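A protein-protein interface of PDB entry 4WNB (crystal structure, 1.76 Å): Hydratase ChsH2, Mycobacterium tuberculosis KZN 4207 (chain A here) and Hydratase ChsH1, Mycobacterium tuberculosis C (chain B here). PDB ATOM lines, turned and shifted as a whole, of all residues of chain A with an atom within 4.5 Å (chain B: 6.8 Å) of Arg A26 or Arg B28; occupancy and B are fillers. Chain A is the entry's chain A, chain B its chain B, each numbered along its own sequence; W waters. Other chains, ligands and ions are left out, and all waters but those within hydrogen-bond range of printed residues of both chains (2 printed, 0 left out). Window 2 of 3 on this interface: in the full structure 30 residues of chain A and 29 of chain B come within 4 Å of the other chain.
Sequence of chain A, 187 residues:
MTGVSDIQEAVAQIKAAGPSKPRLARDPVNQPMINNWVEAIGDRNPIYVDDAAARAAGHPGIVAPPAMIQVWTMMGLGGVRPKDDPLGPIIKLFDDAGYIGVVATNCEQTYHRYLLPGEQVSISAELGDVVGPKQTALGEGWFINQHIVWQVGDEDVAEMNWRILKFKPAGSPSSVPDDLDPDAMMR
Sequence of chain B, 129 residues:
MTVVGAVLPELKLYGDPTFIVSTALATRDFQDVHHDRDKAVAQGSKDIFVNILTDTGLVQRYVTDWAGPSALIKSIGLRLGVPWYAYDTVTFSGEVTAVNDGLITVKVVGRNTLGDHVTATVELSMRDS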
ATOM      1  N   LEU A  24      -3.571 -13.201  13.925  1.00  0.00           N
ATOM      2  CA  LEU A  24      -3.443 -12.820  12.519  1.00  0.00           C
ATOM      3  C   LEU A  24      -4.567 -13.365  11.639  1.00  0.00           C
ATOM      4  O   LEU A  24      -4.981 -14.514  11.782  1.00  0.00           O
ATOM      5  CB  LEU A  24      -2.096 -13.293  11.964  1.00  0.00           C
ATOM      6  CG  LEU A  24      -0.858 -12.440  12.258  1.00  0.00           C
ATOM      7  CD1 LEU A  24      -0.357 -12.620  13.688  1.00  0.00           C
ATOM      8  CD2 LEU A  24       0.242 -12.746  11.248  1.00  0.00           C
ATOM      9  N   ALA A  25      -5.046 -12.529  10.723  1.00  0.00           N
ATOM     10  CA  ALA A  25      -6.021 -12.939   9.710  1.00  0.00           C
ATOM     11  C   ALA A  25      -5.460 -14.081   8.861  1.00  0.00           C
ATOM     12  O   ALA A  25      -4.247 -14.136   8.622  1.00  0.00           O
ATOM     13  CB  ALA A  25      -6.379 -11.757   8.826  1.00  0.00           C
ATOM     14  N   ARG A  26      -6.321 -14.992   8.414  1.00  0.00           N
ATOM     15  CA  ARG A  26      -5.874 -16.109   7.571  1.00  0.00           C
ATOM     16  C   ARG A  26      -5.082 -15.618   6.363  1.00  0.00           C
ATOM     17  O   ARG A  26      -4.033 -16.167   6.035  1.00  0.00           O
ATOM     18  CB  ARG A  26      -7.052 -16.949   7.066  1.00  0.00           C
ATOM     19  CG  ARG A  26      -6.628 -18.310   6.495  1.00  0.00           C
ATOM     20  CD  ARG A  26      -7.800 -19.016   5.846  1.00  0.00           C
ATOM     21  NE  ARG A  26      -8.320 -18.189   4.764  1.00  0.00           N
ATOM     22  CZ  ARG A  26      -9.358 -18.510   3.999  1.00  0.00           C
ATOM     23  NH1 ARG A  26     -10.011 -19.648   4.196  1.00  0.00           N
ATOM     24  NH2 ARG A  26      -9.739 -17.679   3.041  1.00  0.00           N
ATOM     25  N   ASP A  27      -5.607 -14.590   5.708  1.00  0.00           N
ATOM     26  CA  ASP A  27      -4.994 -14.000   4.525  1.00  0.00           C
ATOM     27  C   ASP A  27      -4.796 -12.519   4.718  1.00  0.00           C
ATOM     28  O   ASP A  27      -5.531 -11.897   5.482  1.00  0.00           O
ATOM     29  CB  ASP A  27      -5.861 -14.190   3.275  1.00  0.00           C
ATOM     30  CG  ASP A  27      -6.613 -15.486   3.277  1.00  0.00           C
ATOM     31  OD1 ASP A  27      -6.028 -16.525   2.905  1.00  0.00           O
ATOM     32  OD2 ASP A  27      -7.799 -15.452   3.648  1.00  0.00           O
ATOM     33  N   MET A  33     -11.046 -12.061  -2.446  1.00  0.00           N
ATOM     34  CA  MET A  33     -12.098 -12.020  -1.428  1.00  0.00           C
ATOM     35  C   MET A  33     -12.865 -10.699  -1.470  1.00  0.00           C
ATOM     36  O   MET A  33     -14.061 -10.666  -1.174  1.00  0.00           O
ATOM     37  CB  MET A  33     -11.519 -12.278  -0.033  1.00  0.00           C
ATOM     38  CG  MET A  33     -11.128 -13.729   0.155  1.00  0.00           C
ATOM     39  SD  MET A  33     -10.331 -13.997   1.737  1.00  0.00           S
ATOM     40  CE  MET A  33     -11.430 -13.071   2.826  1.00  0.00           C
ATOM     41  N   VAL A  71     -14.304  -9.369   8.226  1.00  0.00           N
ATOM     42  CA  VAL A  71     -14.215 -10.560   7.378  1.00  0.00           C
ATOM     43  C   VAL A  71     -12.811 -11.204   7.394  1.00  0.00           C
ATOM     44  O   VAL A  71     -12.688 -12.433   7.418  1.00  0.00           O
ATOM     45  CB  VAL A  71     -14.608 -10.213   5.909  1.00  0.00           C
ATOM     46  CG1 VAL A  71     -14.448 -11.430   4.981  1.00  0.00           C
ATOM     47  CG2 VAL A  71     -16.034  -9.692   5.858  1.00  0.00           C
ATOM     48  N   TRP A  72     -11.756 -10.379   7.389  1.00  0.00           N
ATOM     49  CA  TRP A  72     -10.397 -10.904   7.270  1.00  0.00           C
ATOM     50  C   TRP A  72     -10.043 -11.846   8.426  1.00  0.00           C
ATOM     51  O   TRP A  72      -9.343 -12.836   8.226  1.00  0.00           O
ATOM     52  CB  TRP A  72      -9.372  -9.747   7.172  1.00  0.00           C
ATOM     53  CG  TRP A  72      -9.750  -8.721   6.145  1.00  0.00           C
ATOM     54  CD1 TRP A  72     -10.111  -7.430   6.364  1.00  0.00           C
ATOM     55  CD2 TRP A  72      -9.876  -8.939   4.731  1.00  0.00           C
ATOM     56  NE1 TRP A  72     -10.417  -6.810   5.174  1.00  0.00           N
ATOM     57  CE2 TRP A  72     -10.286  -7.721   4.156  1.00  0.00           C
ATOM     58  CE3 TRP A  72      -9.660 -10.037   3.901  1.00  0.00           C
ATOM     59  CZ2 TRP A  72     -10.523  -7.581   2.796  1.00  0.00           C
ATOM     60  CZ3 TRP A  72      -9.877  -9.893   2.546  1.00  0.00           C
ATOM     61  CH2 TRP A  72     -10.298  -8.671   2.004  1.00  0.00           C
ATOM     62  N   MET A  74     -12.326 -13.535  10.503  1.00  0.00           N
ATOM     63  CA  MET A  74     -13.331 -14.532  10.855  1.00  0.00           C
ATOM     64  C   MET A  74     -12.644 -15.880  11.019  1.00  0.00           C
ATOM     65  O   MET A  74     -11.704 -16.197  10.288  1.00  0.00           O
ATOM     66  CB  MET A  74     -14.446 -14.603   9.789  1.00  0.00           C
ATOM     67  CG  MET A  74     -15.313 -13.363   9.774  1.00  0.00           C
ATOM     68  SD  MET A  74     -16.318 -13.179  11.259  1.00  0.00           S
ATOM     69  CE  MET A  74     -17.547 -14.438  10.849  1.00  0.00           C
ATOM     70  N   GLY A  76     -13.593 -18.926  10.381  1.00  0.00           N
ATOM     71  CA  GLY A  76     -13.689 -19.873   9.292  1.00  0.00           C
ATOM     72  C   GLY A  76     -14.444 -21.130   9.672  1.00  0.00           C
ATOM     73  O   GLY A  76     -14.881 -21.307  10.817  1.00  0.00           O
ATOM     74  N   LEU A  77     -14.570 -22.022   8.706  1.00  0.00           N
ATOM     75  CA  LEU A  77     -15.338 -23.235   8.888  1.00  0.00           C
ATOM     76  C   LEU A  77     -14.743 -24.079  10.017  1.00  0.00           C
ATOM     77  O   LEU A  77     -13.573 -24.452   9.974  1.00  0.00           O
ATOM     78  CB  LEU A  77     -15.371 -23.998   7.571  1.00  0.00           C
ATOM     79  CG  LEU A  77     -16.490 -24.987   7.314  1.00  0.00           C
ATOM     80  CD1 LEU A  77     -17.840 -24.369   7.640  1.00  0.00           C
ATOM     81  CD2 LEU A  77     -16.408 -25.405   5.846  1.00  0.00           C
ATOM     82  N   GLN A 120      -1.818  -7.043   6.046  1.00  0.00           N
ATOM     83  CA  GLN A 120      -2.358  -8.116   6.857  1.00  0.00           C
ATOM     84  C   GLN A 120      -2.724  -7.621   8.252  1.00  0.00           C
ATOM     85  O   GLN A 120      -1.941  -6.956   8.954  1.00  0.00           O
ATOM     86  CB  GLN A 120      -1.391  -9.291   6.956  1.00  0.00           C
ATOM     87  CG  GLN A 120      -2.031 -10.567   7.518  1.00  0.00           C
ATOM     88  CD  GLN A 120      -1.319 -11.832   7.057  1.00  0.00           C
ATOM     89  OE1 GLN A 120      -0.246 -11.769   6.456  1.00  0.00           O
ATOM     90  NE2 GLN A 120      -1.913 -12.981   7.331  1.00  0.00           N
ATOM     91  N   THR B  23     -24.145 -13.849   0.601  1.00  0.00           N
ATOM     92  CA  THR B  23     -23.575 -12.757   1.389  1.00  0.00           C
ATOM     93  C   THR B  23     -22.961 -13.322   2.680  1.00  0.00           C
ATOM     94  O   THR B  23     -21.860 -12.913   3.060  1.00  0.00           O
ATOM     95  CB  THR B  23     -24.607 -11.659   1.710  1.00  0.00           C
ATOM     96  OG1 THR B  23     -25.762 -12.249   2.332  1.00  0.00           O
ATOM     97  CG2 THR B  23     -25.016 -10.948   0.434  1.00  0.00           C
ATOM     98  N   ALA B  24     -23.648 -14.242   3.358  1.00  0.00           N
ATOM     99  CA  ALA B  24     -23.071 -14.764   4.601  1.00  0.00           C
ATOM    100  C   ALA B  24     -21.700 -15.406   4.327  1.00  0.00           C
ATOM    101  O   ALA B  24     -20.737 -15.151   5.049  1.00  0.00           O
ATOM    102  CB  ALA B  24     -24.013 -15.775   5.273  1.00  0.00           C
ATOM    103  N   LEU B  25     -21.599 -16.215   3.273  1.00  0.00           N
ATOM    104  CA  LEU B  25     -20.336 -16.919   3.054  1.00  0.00           C
ATOM    105  C   LEU B  25     -19.272 -15.962   2.511  1.00  0.00           C
ATOM    106  O   LEU B  25     -18.079 -16.154   2.786  1.00  0.00           O
ATOM    107  CB  LEU B  25     -20.531 -18.135   2.131  1.00  0.00           C
ATOM    108  CG  LEU B  25     -20.740 -19.442   2.927  1.00  0.00           C
ATOM    109  CD1 LEU B  25     -22.051 -19.389   3.707  1.00  0.00           C
ATOM    110  CD2 LEU B  25     -20.710 -20.663   2.011  1.00  0.00           C
ATOM    111  N   ALA B  26     -19.685 -14.923   1.777  1.00  0.00           N
ATOM    112  CA  ALA B  26     -18.719 -13.888   1.350  1.00  0.00           C
ATOM    113  C   ALA B  26     -18.186 -13.044   2.534  1.00  0.00           C
ATOM    114  O   ALA B  26     -17.110 -12.434   2.417  1.00  0.00           O
ATOM    115  CB  ALA B  26     -19.333 -12.965   0.299  1.00  0.00           C
ATOM    116  N   THR B  27     -18.916 -13.021   3.652  1.00  0.00           N
ATOM    117  CA  THR B  27     -18.407 -12.359   4.868  1.00  0.00           C
ATOM    118  C   THR B  27     -17.725 -13.381   5.796  1.00  0.00           C
ATOM    119  O   THR B  27     -17.353 -13.053   6.928  1.00  0.00           O
ATOM    120  CB  THR B  27     -19.505 -11.618   5.650  1.00  0.00           C
ATOM    121  OG1 THR B  27     -20.493 -12.544   6.130  1.00  0.00           O
ATOM    122  CG2 THR B  27     -20.166 -10.561   4.769  1.00  0.00           C
ATOM    123  N   ARG B  28     -17.540 -14.591   5.266  1.00  0.00           N
ATOM    124  CA  ARG B  28     -16.888 -15.732   5.934  1.00  0.00           C
ATOM    125  C   ARG B  28     -17.557 -16.063   7.262  1.00  0.00           C
ATOM    126  O   ARG B  28     -16.905 -16.424   8.251  1.00  0.00           O
ATOM    127  CB  ARG B  28     -15.376 -15.498   6.104  1.00  0.00           C
ATOM    128  CG  ARG B  28     -14.614 -15.730   4.776  1.00  0.00           C
ATOM    129  CD  ARG B  28     -13.103 -15.949   4.918  1.00  0.00           C
ATOM    130  NE  ARG B  28     -12.717 -17.088   5.759  1.00  0.00           N
ATOM    131  CZ  ARG B  28     -12.871 -18.367   5.429  1.00  0.00           C
ATOM    132  NH1 ARG B  28     -13.445 -18.712   4.282  1.00  0.00           N
ATOM    133  NH2 ARG B  28     -12.465 -19.309   6.264  1.00  0.00           N
ATOM    134  N   ASP B  29     -18.888 -15.990   7.235  1.00  0.00           N
ATOM    135  CA  ASP B  29     -19.732 -16.314   8.365  1.00  0.00           C
ATOM    136  C   ASP B  29     -20.422 -17.648   8.042  1.00  0.00           C
ATOM    137  O   ASP B  29     -21.330 -17.692   7.202  1.00  0.00           O
ATOM    138  CB  ASP B  29     -20.776 -15.200   8.576  1.00  0.00           C
ATOM    139  CG  ASP B  29     -21.646 -15.396   9.809  1.00  0.00           C
ATOM    140  OD1 ASP B  29     -21.795 -16.521  10.330  1.00  0.00           O
ATOM    141  OD2 ASP B  29     -22.212 -14.365  10.208  1.00  0.00           O
ATOM    142  N   PHE B  30     -19.979 -18.721   8.695  1.00  0.00           N
ATOM    143  CA  PHE B  30     -20.458 -20.051   8.357  1.00  0.00           C
ATOM    144  C   PHE B  30     -21.490 -20.553   9.384  1.00  0.00           C
ATOM    145  O   PHE B  30     -21.813 -21.758   9.405  1.00  0.00           O
ATOM    146  CB  PHE B  30     -19.271 -21.007   8.258  1.00  0.00           C
ATOM    147  CG  PHE B  30     -18.390 -20.761   7.049  1.00  0.00           C
ATOM    148  CD1 PHE B  30     -18.671 -21.365   5.826  1.00  0.00           C
ATOM    149  CD2 PHE B  30     -17.320 -19.902   7.135  1.00  0.00           C
ATOM    150  CE1 PHE B  30     -17.863 -21.126   4.704  1.00  0.00           C
ATOM    151  CE2 PHE B  30     -16.506 -19.654   6.024  1.00  0.00           C
ATOM    152  CZ  PHE B  30     -16.783 -20.267   4.809  1.00  0.00           C
ATOM    153  N   GLN B  31     -22.028 -19.650  10.209  1.00  0.00           N
ATOM    154  CA  GLN B  31     -23.073 -20.046  11.179  1.00  0.00           C
ATOM    155  C   GLN B  31     -24.223 -20.704  10.438  1.00  0.00           C
ATOM    156  O   GLN B  31     -24.679 -20.197   9.406  1.00  0.00           O
ATOM    157  CB  GLN B  31     -23.661 -18.867  11.981  1.00  0.00           C
ATOM    158  CG  GLN B  31     -22.770 -18.036  12.877  1.00  0.00           C
ATOM    159  CD  GLN B  31     -23.623 -17.046  13.705  1.00  0.00           C
ATOM    160  OE1 GLN B  31     -24.817 -17.260  13.884  1.00  0.00           O
ATOM    161  NE2 GLN B  31     -23.011 -15.988  14.196  1.00  0.00           N
ATOM    162  N   ASN B  51     -27.088 -12.068   7.881  1.00  0.00           N
ATOM    163  CA  ASN B  51     -26.173 -11.916   9.010  1.00  0.00           C
ATOM    164  C   ASN B  51     -25.789 -10.450   9.246  1.00  0.00           C
ATOM    165  O   ASN B  51     -26.103  -9.571   8.449  1.00  0.00           O
ATOM    166  CB  ASN B  51     -24.922 -12.811   8.825  1.00  0.00           C
ATOM    167  CG  ASN B  51     -23.873 -12.223   7.883  1.00  0.00           C
ATOM    168  OD1 ASN B  51     -24.187 -11.475   6.974  1.00  0.00           O
ATOM    169  ND2 ASN B  51     -22.605 -12.592   8.102  1.00  0.00           N
ATOM    170  N   LEU B  53     -22.833  -8.939   9.413  1.00  0.00           N
ATOM    171  CA  LEU B  53     -21.781  -8.376   8.559  1.00  0.00           C
ATOM    172  C   LEU B  53     -22.342  -7.932   7.215  1.00  0.00           C
ATOM    173  O   LEU B  53     -21.842  -6.985   6.616  1.00  0.00           O
ATOM    174  CB  LEU B  53     -20.640  -9.368   8.353  1.00  0.00           C
ATOM    175  CG  LEU B  53     -19.502  -9.229   9.368  1.00  0.00           C
ATOM    176  CD1 LEU B  53     -18.387 -10.260   9.169  1.00  0.00           C
ATOM    177  CD2 LEU B  53     -18.946  -7.797   9.331  1.00  0.00           C
HETATM  178  O   HOH W   1     -14.997 -12.793   0.677  1.00  0.00           O
HETATM  179  O   HOH W   2     -16.176 -17.743  10.572  1.00  0.00           O
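The guanidinium group of Arg A26 sits close to the guanidinium group of Arg B28.
OG1 of Thr B27 lies close to O of Thr B23 (3.4 Å).
OG1 of Thr B27 lies within hydrogen-bond range of ND2 of Asn B51, 2.9 Å away.
N of Asp B29 sits at hydrogen-bond distance from O of Ala B24, 3.0 Å away.
The backbone carbonyl oxygen (O) of Ala B24 sits at hydrogen-bond distance from the side-chain hydroxyl (OG1) of Thr B27 (2.8 Å).
The side-chain carboxylate (OD2) of Asp B29 lies close to the side-chain amide nitrogen (ND2) of Asn B51 (2.8 Å).
NE of Arg A26 lies within salt-bridge range of OD2 of Asp A27 (3.0 Å).
Water W1 bridges the backbone carbonyl oxygen of Ala B26 (2.8 Å) and the backbone carbonyl oxygen of Met A33 (3.0 Å).
Water W2 bridges O of Arg B28 (2.8 Å) and N of Gly A76 (2.8 Å).
Of the 11 printed residues of chain B, 5 touch a printed residue of chain A.
Hydrophobic or aromatic side chains of chain A that line the printed part of chain B: Met A33, Val A71, Met A74 and Leu A77.
Among the printed residues, 9 pairs touch across the chains.
Among the printed residues, no Asp or Glu carboxylate lies within 4 Å of a Lys or Arg side-chain nitrogen of the other chain.
Among the printed residues, merely in contact across the chains: Gly A76 with Arg B28 (3.3 Å), Met A74 with Arg B28 (3.3 Å), Met A74 with Thr B27 (3.5 Å), Leu A77 with Phe B30 (3.6 Å), Val A71 with Thr B27 (3.7 Å), Met A74 with Asp B29 (3.8 Å), Val A71 with Ala B26 (3.8 Å) and Met A33 with Arg B28 (3.9 Å).
Printed residues of chain B within 4 Å of Arg A26: Arg B28.
Of the printed residues of chain B, Met A33 touches Arg B28.
Of the printed residues of chain B, Leu A77 touches Phe B30.
Gln A120 touches none of the printed residues of chain B.
Leu B25 touches none of the printed residues of chain A.
Of the printed residues of chain A, Arg B28 touches Arg A26 (3.2 Å), Met A33 (3.9 Å), Met A74 (3.3 Å) and Gly A76 (3.3 Å).
The nearest printed residue of chain B that does not touch Met A74 is Leu B53 (4.1 Å).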
